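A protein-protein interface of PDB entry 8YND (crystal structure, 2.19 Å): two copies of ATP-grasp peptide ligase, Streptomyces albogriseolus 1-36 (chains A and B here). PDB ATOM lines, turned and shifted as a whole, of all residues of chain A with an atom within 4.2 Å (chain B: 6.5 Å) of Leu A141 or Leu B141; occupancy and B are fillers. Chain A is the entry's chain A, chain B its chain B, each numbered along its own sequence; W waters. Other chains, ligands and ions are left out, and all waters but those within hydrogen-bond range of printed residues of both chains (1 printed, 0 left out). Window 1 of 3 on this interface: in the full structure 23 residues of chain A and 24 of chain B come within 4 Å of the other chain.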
ATOM      1  N   ASN A 137      17.448 -30.122 -16.588  1.00  0.00           N
ATOM      2  CA  ASN A 137      17.041 -31.380 -15.958  1.00  0.00           C
ATOM      3  C   ASN A 137      15.578 -31.335 -15.526  1.00  0.00           C
ATOM      4  O   ASN A 137      15.212 -31.714 -14.409  1.00  0.00           O
ATOM      5  CB  ASN A 137      17.963 -31.744 -14.790  1.00  0.00           C
ATOM      6  CG  ASN A 137      19.312 -32.266 -15.273  1.00  0.00           C
ATOM      7  OD1 ASN A 137      19.397 -33.314 -15.945  1.00  0.00           O
ATOM      8  ND2 ASN A 137      20.366 -31.518 -14.971  1.00  0.00           N
ATOM      9  N   GLY A 138      14.740 -30.890 -16.458  1.00  0.00           N
ATOM     10  CA  GLY A 138      13.322 -30.820 -16.190  1.00  0.00           C
ATOM     11  C   GLY A 138      12.736 -32.158 -15.820  1.00  0.00           C
ATOM     12  O   GLY A 138      11.835 -32.227 -14.981  1.00  0.00           O
ATOM     13  N   ILE A 139      13.239 -33.240 -16.423  1.00  0.00           N
ATOM     14  CA  ILE A 139      12.565 -34.514 -16.227  1.00  0.00           C
ATOM     15  C   ILE A 139      12.914 -35.114 -14.871  1.00  0.00           C
ATOM     16  O   ILE A 139      12.186 -35.987 -14.385  1.00  0.00           O
ATOM     17  CB  ILE A 139      12.836 -35.481 -17.399  1.00  0.00           C
ATOM     18  CG1 ILE A 139      14.210 -36.109 -17.302  1.00  0.00           C
ATOM     19  CG2 ILE A 139      12.662 -34.795 -18.761  1.00  0.00           C
ATOM     20  CD1 ILE A 139      14.134 -37.424 -16.710  1.00  0.00           C
ATOM     21  N   ASP A 140      13.997 -34.670 -14.234  1.00  0.00           N
ATOM     22  CA  ASP A 140      14.164 -34.970 -12.814  1.00  0.00           C
ATOM     23  C   ASP A 140      12.983 -34.442 -12.000  1.00  0.00           C
ATOM     24  O   ASP A 140      12.474 -35.135 -11.110  1.00  0.00           O
ATOM     25  CB  ASP A 140      15.469 -34.377 -12.276  1.00  0.00           C
ATOM     26  CG  ASP A 140      16.664 -35.264 -12.524  1.00  0.00           C
ATOM     27  OD1 ASP A 140      16.476 -36.496 -12.671  1.00  0.00           O
ATOM     28  OD2 ASP A 140      17.803 -34.727 -12.547  1.00  0.00           O
ATOM     29  N   LEU A 141      12.548 -33.209 -12.278  1.00  0.00           N
ATOM     30  CA  LEU A 141      11.386 -32.671 -11.581  1.00  0.00           C
ATOM     31  C   LEU A 141      10.176 -33.579 -11.751  1.00  0.00           C
ATOM     32  O   LEU A 141       9.520 -33.936 -10.770  1.00  0.00           O
ATOM     33  CB  LEU A 141      11.061 -31.265 -12.082  1.00  0.00           C
ATOM     34  CG  LEU A 141      10.008 -30.473 -11.295  1.00  0.00           C
ATOM     35  CD1 LEU A 141      10.302 -30.508  -9.796  1.00  0.00           C
ATOM     36  CD2 LEU A 141       9.937 -29.043 -11.834  1.00  0.00           C
ATOM     37  N   LEU A 142       9.888 -33.992 -12.992  1.00  0.00           N
ATOM     38  CA  LEU A 142       8.690 -34.777 -13.267  1.00  0.00           C
ATOM     39  C   LEU A 142       8.762 -36.182 -12.676  1.00  0.00           C
ATOM     40  O   LEU A 142       7.725 -36.768 -12.357  1.00  0.00           O
ATOM     41  CB  LEU A 142       8.456 -34.867 -14.778  1.00  0.00           C
ATOM     42  CG  LEU A 142       8.293 -33.550 -15.546  1.00  0.00           C
ATOM     43  CD1 LEU A 142       8.422 -33.771 -17.032  1.00  0.00           C
ATOM     44  CD2 LEU A 142       6.976 -32.917 -15.239  1.00  0.00           C
ATOM     45  N   ASN A 143       9.954 -36.748 -12.535  1.00  0.00           N
ATOM     46  CA  ASN A 143      10.090 -38.116 -12.081  1.00  0.00           C
ATOM     47  C   ASN A 143      10.186 -38.236 -10.569  1.00  0.00           C
ATOM     48  O   ASN A 143      10.701 -39.236 -10.067  1.00  0.00           O
ATOM     49  CB  ASN A 143      11.304 -38.755 -12.748  1.00  0.00           C
ATOM     50  CG  ASN A 143      10.984 -39.240 -14.130  1.00  0.00           C
ATOM     51  OD1 ASN A 143       9.822 -39.482 -14.450  1.00  0.00           O
ATOM     52  ND2 ASN A 143      11.996 -39.351 -14.971  1.00  0.00           N
ATOM     53  N   MET A 144       9.731 -37.230  -9.841  1.00  0.00           N
ATOM     54  CA  MET A 144       9.623 -37.285  -8.397  1.00  0.00           C
ATOM     55  C   MET A 144       8.191 -37.627  -8.022  1.00  0.00           C
ATOM     56  O   MET A 144       7.246 -37.192  -8.686  1.00  0.00           O
ATOM     57  CB  MET A 144      10.035 -35.949  -7.781  1.00  0.00           C
ATOM     58  CG  MET A 144      11.509 -35.615  -7.950  1.00  0.00           C
ATOM     59  SD  MET A 144      11.764 -33.892  -7.573  1.00  0.00           S
ATOM     60  CE  MET A 144      11.839 -34.030  -5.774  1.00  0.00           C
ATOM     61  N   THR A 147       6.256 -34.454  -6.834  1.00  0.00           N
ATOM     62  CA  THR A 147       5.817 -33.631  -7.959  1.00  0.00           C
ATOM     63  C   THR A 147       4.515 -34.151  -8.549  1.00  0.00           C
ATOM     64  O   THR A 147       3.626 -33.366  -8.896  1.00  0.00           O
ATOM     65  CB  THR A 147       6.908 -33.615  -9.035  1.00  0.00           C
ATOM     66  OG1 THR A 147       8.072 -32.942  -8.544  1.00  0.00           O
ATOM     67  CG2 THR A 147       6.429 -32.945 -10.311  1.00  0.00           C
ATOM     68  N   ARG A 150       1.568 -33.332  -6.196  1.00  0.00           N
ATOM     69  CA  ARG A 150       1.267 -31.901  -6.228  1.00  0.00           C
ATOM     70  C   ARG A 150       0.552 -31.510  -7.516  1.00  0.00           C
ATOM     71  O   ARG A 150      -0.536 -30.912  -7.491  1.00  0.00           O
ATOM     72  CB  ARG A 150       2.566 -31.113  -6.081  1.00  0.00           C
ATOM     73  CG  ARG A 150       3.108 -31.061  -4.660  1.00  0.00           C
ATOM     74  CD  ARG A 150       4.587 -30.715  -4.718  1.00  0.00           C
ATOM     75  NE  ARG A 150       5.192 -30.622  -3.397  1.00  0.00           N
ATOM     76  CZ  ARG A 150       6.490 -30.460  -3.158  1.00  0.00           C
ATOM     77  NH1 ARG A 150       7.387 -30.465  -4.132  1.00  0.00           N
ATOM     78  NH2 ARG A 150       6.898 -30.289  -1.908  1.00  0.00           N
ATOM     79  N   PHE B 133      -4.082 -28.687  -3.654  1.00  0.00           N
ATOM     80  CA  PHE B 133      -2.713 -28.321  -4.012  1.00  0.00           C
ATOM     81  C   PHE B 133      -1.942 -27.832  -2.790  1.00  0.00           C
ATOM     82  O   PHE B 133      -0.785 -28.219  -2.579  1.00  0.00           O
ATOM     83  CB  PHE B 133      -2.753 -27.259  -5.122  1.00  0.00           C
ATOM     84  CG  PHE B 133      -1.407 -26.890  -5.696  1.00  0.00           C
ATOM     85  CD1 PHE B 133      -0.706 -27.784  -6.503  1.00  0.00           C
ATOM     86  CD2 PHE B 133      -0.880 -25.623  -5.487  1.00  0.00           C
ATOM     87  CE1 PHE B 133       0.508 -27.437  -7.053  1.00  0.00           C
ATOM     88  CE2 PHE B 133       0.335 -25.265  -6.023  1.00  0.00           C
ATOM     89  CZ  PHE B 133       1.037 -26.169  -6.809  1.00  0.00           C
ATOM     90  N   ASN B 137       1.454 -29.216  -0.308  1.00  0.00           N
ATOM     91  CA  ASN B 137       2.516 -28.216  -0.239  1.00  0.00           C
ATOM     92  C   ASN B 137       3.056 -27.892  -1.632  1.00  0.00           C
ATOM     93  O   ASN B 137       4.264 -27.722  -1.835  1.00  0.00           O
ATOM     94  CB  ASN B 137       3.625 -28.645   0.726  1.00  0.00           C
ATOM     95  CG  ASN B 137       3.211 -28.480   2.184  1.00  0.00           C
ATOM     96  OD1 ASN B 137       2.746 -27.410   2.604  1.00  0.00           O
ATOM     97  ND2 ASN B 137       3.397 -29.525   2.964  1.00  0.00           N
ATOM     98  N   GLY B 138       2.125 -27.772  -2.585  1.00  0.00           N
ATOM     99  CA  GLY B 138       2.476 -27.385  -3.935  1.00  0.00           C
ATOM    100  C   GLY B 138       3.143 -26.028  -4.025  1.00  0.00           C
ATOM    101  O   GLY B 138       4.003 -25.821  -4.876  1.00  0.00           O
ATOM    102  N   ILE B 139       2.773 -25.096  -3.140  1.00  0.00           N
ATOM    103  CA  ILE B 139       3.409 -23.784  -3.134  1.00  0.00           C
ATOM    104  C   ILE B 139       4.908 -23.906  -2.896  1.00  0.00           C
ATOM    105  O   ILE B 139       5.712 -23.188  -3.507  1.00  0.00           O
ATOM    106  CB  ILE B 139       2.740 -22.870  -2.096  1.00  0.00           C
ATOM    107  CG1 ILE B 139       1.438 -22.295  -2.665  1.00  0.00           C
ATOM    108  CG2 ILE B 139       3.694 -21.730  -1.720  1.00  0.00           C
ATOM    109  CD1 ILE B 139       0.220 -23.185  -2.553  1.00  0.00           C
ATOM    110  N   ASP B 140       5.314 -24.824  -2.021  1.00  0.00           N
ATOM    111  CA  ASP B 140       6.737 -25.083  -1.847  1.00  0.00           C
ATOM    112  C   ASP B 140       7.409 -25.446  -3.171  1.00  0.00           C
ATOM    113  O   ASP B 140       8.570 -25.089  -3.392  1.00  0.00           O
ATOM    114  CB  ASP B 140       6.942 -26.200  -0.828  1.00  0.00           C
ATOM    115  CG  ASP B 140       7.080 -25.688   0.600  1.00  0.00           C
ATOM    116  OD1 ASP B 140       7.247 -24.462   0.813  1.00  0.00           O
ATOM    117  OD2 ASP B 140       7.050 -26.535   1.524  1.00  0.00           O
ATOM    118  N   LEU B 141       6.697 -26.142  -4.067  1.00  0.00           N
ATOM    119  CA  LEU B 141       7.293 -26.542  -5.342  1.00  0.00           C
ATOM    120  C   LEU B 141       7.482 -25.344  -6.269  1.00  0.00           C
ATOM    121  O   LEU B 141       8.530 -25.213  -6.912  1.00  0.00           O
ATOM    122  CB  LEU B 141       6.434 -27.615  -6.017  1.00  0.00           C
ATOM    123  CG  LEU B 141       6.549 -27.818  -7.536  1.00  0.00           C
ATOM    124  CD1 LEU B 141       7.891 -28.380  -7.918  1.00  0.00           C
ATOM    125  CD2 LEU B 141       5.462 -28.725  -8.016  1.00  0.00           C
ATOM    126  N   LEU B 142       6.494 -24.449  -6.339  1.00  0.00           N
ATOM    127  CA  LEU B 142       6.621 -23.299  -7.233  1.00  0.00           C
ATOM    128  C   LEU B 142       7.603 -22.260  -6.718  1.00  0.00           C
ATOM    129  O   LEU B 142       8.125 -21.469  -7.505  1.00  0.00           O
ATOM    130  CB  LEU B 142       5.265 -22.639  -7.433  1.00  0.00           C
ATOM    131  CG  LEU B 142       4.149 -23.588  -7.874  1.00  0.00           C
ATOM    132  CD1 LEU B 142       2.837 -22.825  -7.961  1.00  0.00           C
ATOM    133  CD2 LEU B 142       4.516 -24.247  -9.203  1.00  0.00           C
ATOM    134  N   ASN B 143       7.865 -22.222  -5.421  1.00  0.00           N
ATOM    135  CA  ASN B 143       8.710 -21.183  -4.860  1.00  0.00           C
ATOM    136  C   ASN B 143      10.193 -21.564  -4.839  1.00  0.00           C
ATOM    137  O   ASN B 143      10.936 -21.038  -4.012  1.00  0.00           O
ATOM    138  CB  ASN B 143       8.209 -20.826  -3.460  1.00  0.00           C
ATOM    139  CG  ASN B 143       7.097 -19.800  -3.498  1.00  0.00           C
ATOM    140  OD1 ASN B 143       6.975 -19.060  -4.467  1.00  0.00           O
ATOM    141  ND2 ASN B 143       6.281 -19.746  -2.447  1.00  0.00           N
ATOM    142  N   MET B 144      10.619 -22.486  -5.709  1.00  0.00           N
ATOM    143  CA  MET B 144      12.022 -22.830  -5.924  1.00  0.00           C
ATOM    144  C   MET B 144      12.495 -22.294  -7.268  1.00  0.00           C
ATOM    145  O   MET B 144      11.812 -22.452  -8.289  1.00  0.00           O
ATOM    146  CB  MET B 144      12.254 -24.340  -5.868  1.00  0.00           C
ATOM    147  CG  MET B 144      11.578 -25.041  -4.703  1.00  0.00           C
ATOM    148  SD  MET B 144      11.477 -26.799  -5.055  1.00  0.00           S
ATOM    149  CE  MET B 144      13.182 -27.284  -4.849  1.00  0.00           C
ATOM    150  N   LYS B 145      13.664 -21.661  -7.264  1.00  0.00           N
ATOM    151  CA  LYS B 145      14.203 -21.127  -8.503  1.00  0.00           C
ATOM    152  C   LYS B 145      14.485 -22.234  -9.516  1.00  0.00           C
ATOM    153  O   LYS B 145      14.341 -22.012 -10.727  1.00  0.00           O
ATOM    154  CB  LYS B 145      15.459 -20.304  -8.215  1.00  0.00           C
ATOM    155  CG  LYS B 145      15.225 -19.250  -7.132  1.00  0.00           C
ATOM    156  CD  LYS B 145      16.358 -18.247  -7.097  1.00  0.00           C
ATOM    157  CE  LYS B 145      16.159 -17.246  -5.975  1.00  0.00           C
ATOM    158  NZ  LYS B 145      16.512 -17.888  -4.703  1.00  0.00           N
ATOM    159  N   SER B 146      14.866 -23.429  -9.052  1.00  0.00           N
ATOM    160  CA  SER B 146      15.062 -24.526  -9.997  1.00  0.00           C
ATOM    161  C   SER B 146      13.770 -24.800 -10.769  1.00  0.00           C
ATOM    162  O   SER B 146      13.781 -24.930 -12.004  1.00  0.00           O
ATOM    163  CB  SER B 146      15.539 -25.784  -9.265  1.00  0.00           C
ATOM    164  OG  SER B 146      14.592 -26.191  -8.272  1.00  0.00           O
ATOM    165  N   THR B 147      12.643 -24.848 -10.055  1.00  0.00           N
ATOM    166  CA  THR B 147      11.353 -25.069 -10.691  1.00  0.00           C
ATOM    167  C   THR B 147      11.077 -24.003 -11.735  1.00  0.00           C
ATOM    168  O   THR B 147      10.547 -24.299 -12.813  1.00  0.00           O
ATOM    169  CB  THR B 147      10.236 -25.087  -9.642  1.00  0.00           C
ATOM    170  OG1 THR B 147      10.460 -26.165  -8.722  1.00  0.00           O
ATOM    171  CG2 THR B 147       8.867 -25.265 -10.309  1.00  0.00           C
ATOM    172  N   PHE B 148      11.426 -22.755 -11.442  1.00  0.00           N
ATOM    173  CA  PHE B 148      11.130 -21.710 -12.411  1.00  0.00           C
ATOM    174  C   PHE B 148      11.935 -21.894 -13.696  1.00  0.00           C
ATOM    175  O   PHE B 148      11.387 -21.758 -14.792  1.00  0.00           O
ATOM    176  CB  PHE B 148      11.402 -20.336 -11.830  1.00  0.00           C
ATOM    177  CG  PHE B 148      11.243 -19.259 -12.833  1.00  0.00           C
ATOM    178  CD1 PHE B 148       9.975 -18.820 -13.198  1.00  0.00           C
ATOM    179  CD2 PHE B 148      12.354 -18.710 -13.459  1.00  0.00           C
ATOM    180  CE1 PHE B 148       9.820 -17.832 -14.162  1.00  0.00           C
ATOM    181  CE2 PHE B 148      12.209 -17.722 -14.408  1.00  0.00           C
ATOM    182  CZ  PHE B 148      10.942 -17.281 -14.767  1.00  0.00           C
ATOM    183  N   ARG B 150      13.063 -24.665 -14.935  1.00  0.00           N
ATOM    184  CA  ARG B 150      12.553 -25.829 -15.645  1.00  0.00           C
ATOM    185  C   ARG B 150      11.239 -25.515 -16.352  1.00  0.00           C
ATOM    186  O   ARG B 150      11.083 -25.819 -17.537  1.00  0.00           O
ATOM    187  CB  ARG B 150      12.380 -26.993 -14.672  1.00  0.00           C
ATOM    188  CG  ARG B 150      13.688 -27.453 -14.070  1.00  0.00           C
ATOM    189  CD  ARG B 150      13.495 -28.244 -12.777  1.00  0.00           C
ATOM    190  NE  ARG B 150      14.694 -29.026 -12.506  1.00  0.00           N
ATOM    191  CZ  ARG B 150      14.886 -29.816 -11.455  1.00  0.00           C
ATOM    192  NH1 ARG B 150      14.022 -29.871 -10.457  1.00  0.00           N
ATOM    193  NH2 ARG B 150      15.976 -30.569 -11.410  1.00  0.00           N
ATOM    194  N   LEU B 151      10.270 -24.933 -15.645  1.00  0.00           N
ATOM    195  CA  LEU B 151       9.005 -24.590 -16.294  1.00  0.00           C
ATOM    196  C   LEU B 151       9.216 -23.538 -17.370  1.00  0.00           C
ATOM    197  O   LEU B 151       8.571 -23.574 -18.435  1.00  0.00           O
ATOM    198  CB  LEU B 151       7.982 -24.085 -15.268  1.00  0.00           C
ATOM    199  CG  LEU B 151       7.521 -25.085 -14.197  1.00  0.00           C
ATOM    200  CD1 LEU B 151       6.666 -24.406 -13.149  1.00  0.00           C
ATOM    201  CD2 LEU B 151       6.720 -26.176 -14.847  1.00  0.00           C
ATOM    202  N   ARG B 191      15.734 -21.454  -2.626  1.00  0.00           N
ATOM    203  CA  ARG B 191      14.500 -20.976  -2.005  1.00  0.00           C
ATOM    204  C   ARG B 191      14.611 -19.573  -1.409  1.00  0.00           C
ATOM    205  O   ARG B 191      13.809 -19.215  -0.536  1.00  0.00           O
ATOM    206  CB  ARG B 191      14.062 -21.957  -0.925  1.00  0.00           C
ATOM    207  CG  ARG B 191      14.290 -23.388  -1.312  1.00  0.00           C
ATOM    208  CD  ARG B 191      13.428 -24.339  -0.497  1.00  0.00           C
ATOM    209  NE  ARG B 191      12.057 -24.434  -0.980  1.00  0.00           N
ATOM    210  CZ  ARG B 191      11.415 -25.580  -1.178  1.00  0.00           C
ATOM    211  NH1 ARG B 191      12.021 -26.755  -1.015  1.00  0.00           N
ATOM    212  NH2 ARG B 191      10.138 -25.550  -1.551  1.00  0.00           N
ATOM    213  N   ILE B 316      -1.673 -25.484 -13.469  1.00  0.00           N
ATOM    214  CA  ILE B 316      -1.095 -26.441 -12.534  1.00  0.00           C
ATOM    215  C   ILE B 316      -1.926 -26.528 -11.256  1.00  0.00           C
ATOM    216  O   ILE B 316      -1.985 -27.582 -10.615  1.00  0.00           O
ATOM    217  CB  ILE B 316       0.368 -26.046 -12.239  1.00  0.00           C
ATOM    218  CG1 ILE B 316       1.288 -26.398 -13.421  1.00  0.00           C
ATOM    219  CG2 ILE B 316       0.884 -26.736 -10.985  1.00  0.00           C
ATOM    220  CD1 ILE B 316       2.719 -25.860 -13.261  1.00  0.00           C
HETATM  221  O   HOH W   1      18.373 -32.949 -10.800  1.00  0.00           O
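O of Asn A137 sits at hydrogen-bond distance from NH2 of Arg B150 (3.3 Å). The guanidinium group of Arg A150 sits at hydrogen-bond distance from the backbone carbonyl oxygen of Asn B137 (3.4 Å).
Asn A137 touches Arg B150, and with the chains exchanged Arg A150 touches Asn B137. Gly A138 touches Arg B150, and with the chains exchanged Arg A150 touches Gly B138. Asp A140 touches Arg B150, but with the chains exchanged Arg A150 does not touch Asp B140 (4.2 Å). Leu A141 touches its own counterpart, Leu B141. Positions printed for both chains: 137, 138, 139, 140, 141, 142, 143, 144, 147 and 150.
Leu A141 touches two residues of chain B. Of the printed residues of chain B, Asn A137 touches Arg B150. Of the printed residues of chain B, Asp A140 touches Arg B150. The nearest residue of chain B that does not touch Leu A141 is Thr B147 (4.2 Å).
Water W1 bridges OD2 of Asp A140 (2.6 Å) and NH2 of Arg B150 (3.4 Å).
CA of Gly A138 touches CG of Arg B150, at 3.996 Å. Asp A140 touches Arg B150 (CB to NH2, 3.9 Å). CD1 of Leu B141 touches CD1 of Leu A141, at 3.7 Å. Leu A141 touches Arg B150. Phe B133 touches Arg A150. Arg A150 touches Gly B138 (CG to CA, 3.8 Å). Arg A150 touches Leu B141.
Printed residues of chain A that touch a printed residue of chain B: Asn A137, Gly A138, Asp A140, Leu A141 and Arg A150. Along chain B the printed residues that touch a printed residue of chain A span positions 133 to 150.
O of Leu A141 lies within hydrogen-bond range of OG1 of Thr A147, at 2.8 Å. O of Phe B133 sits at hydrogen-bond distance from N of Gly B138. The backbone carbonyl oxygen (O) of Leu B141 sits at hydrogen-bond distance from the side-chain hydroxyl (OG1) of Thr B147 (2.8 Å).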
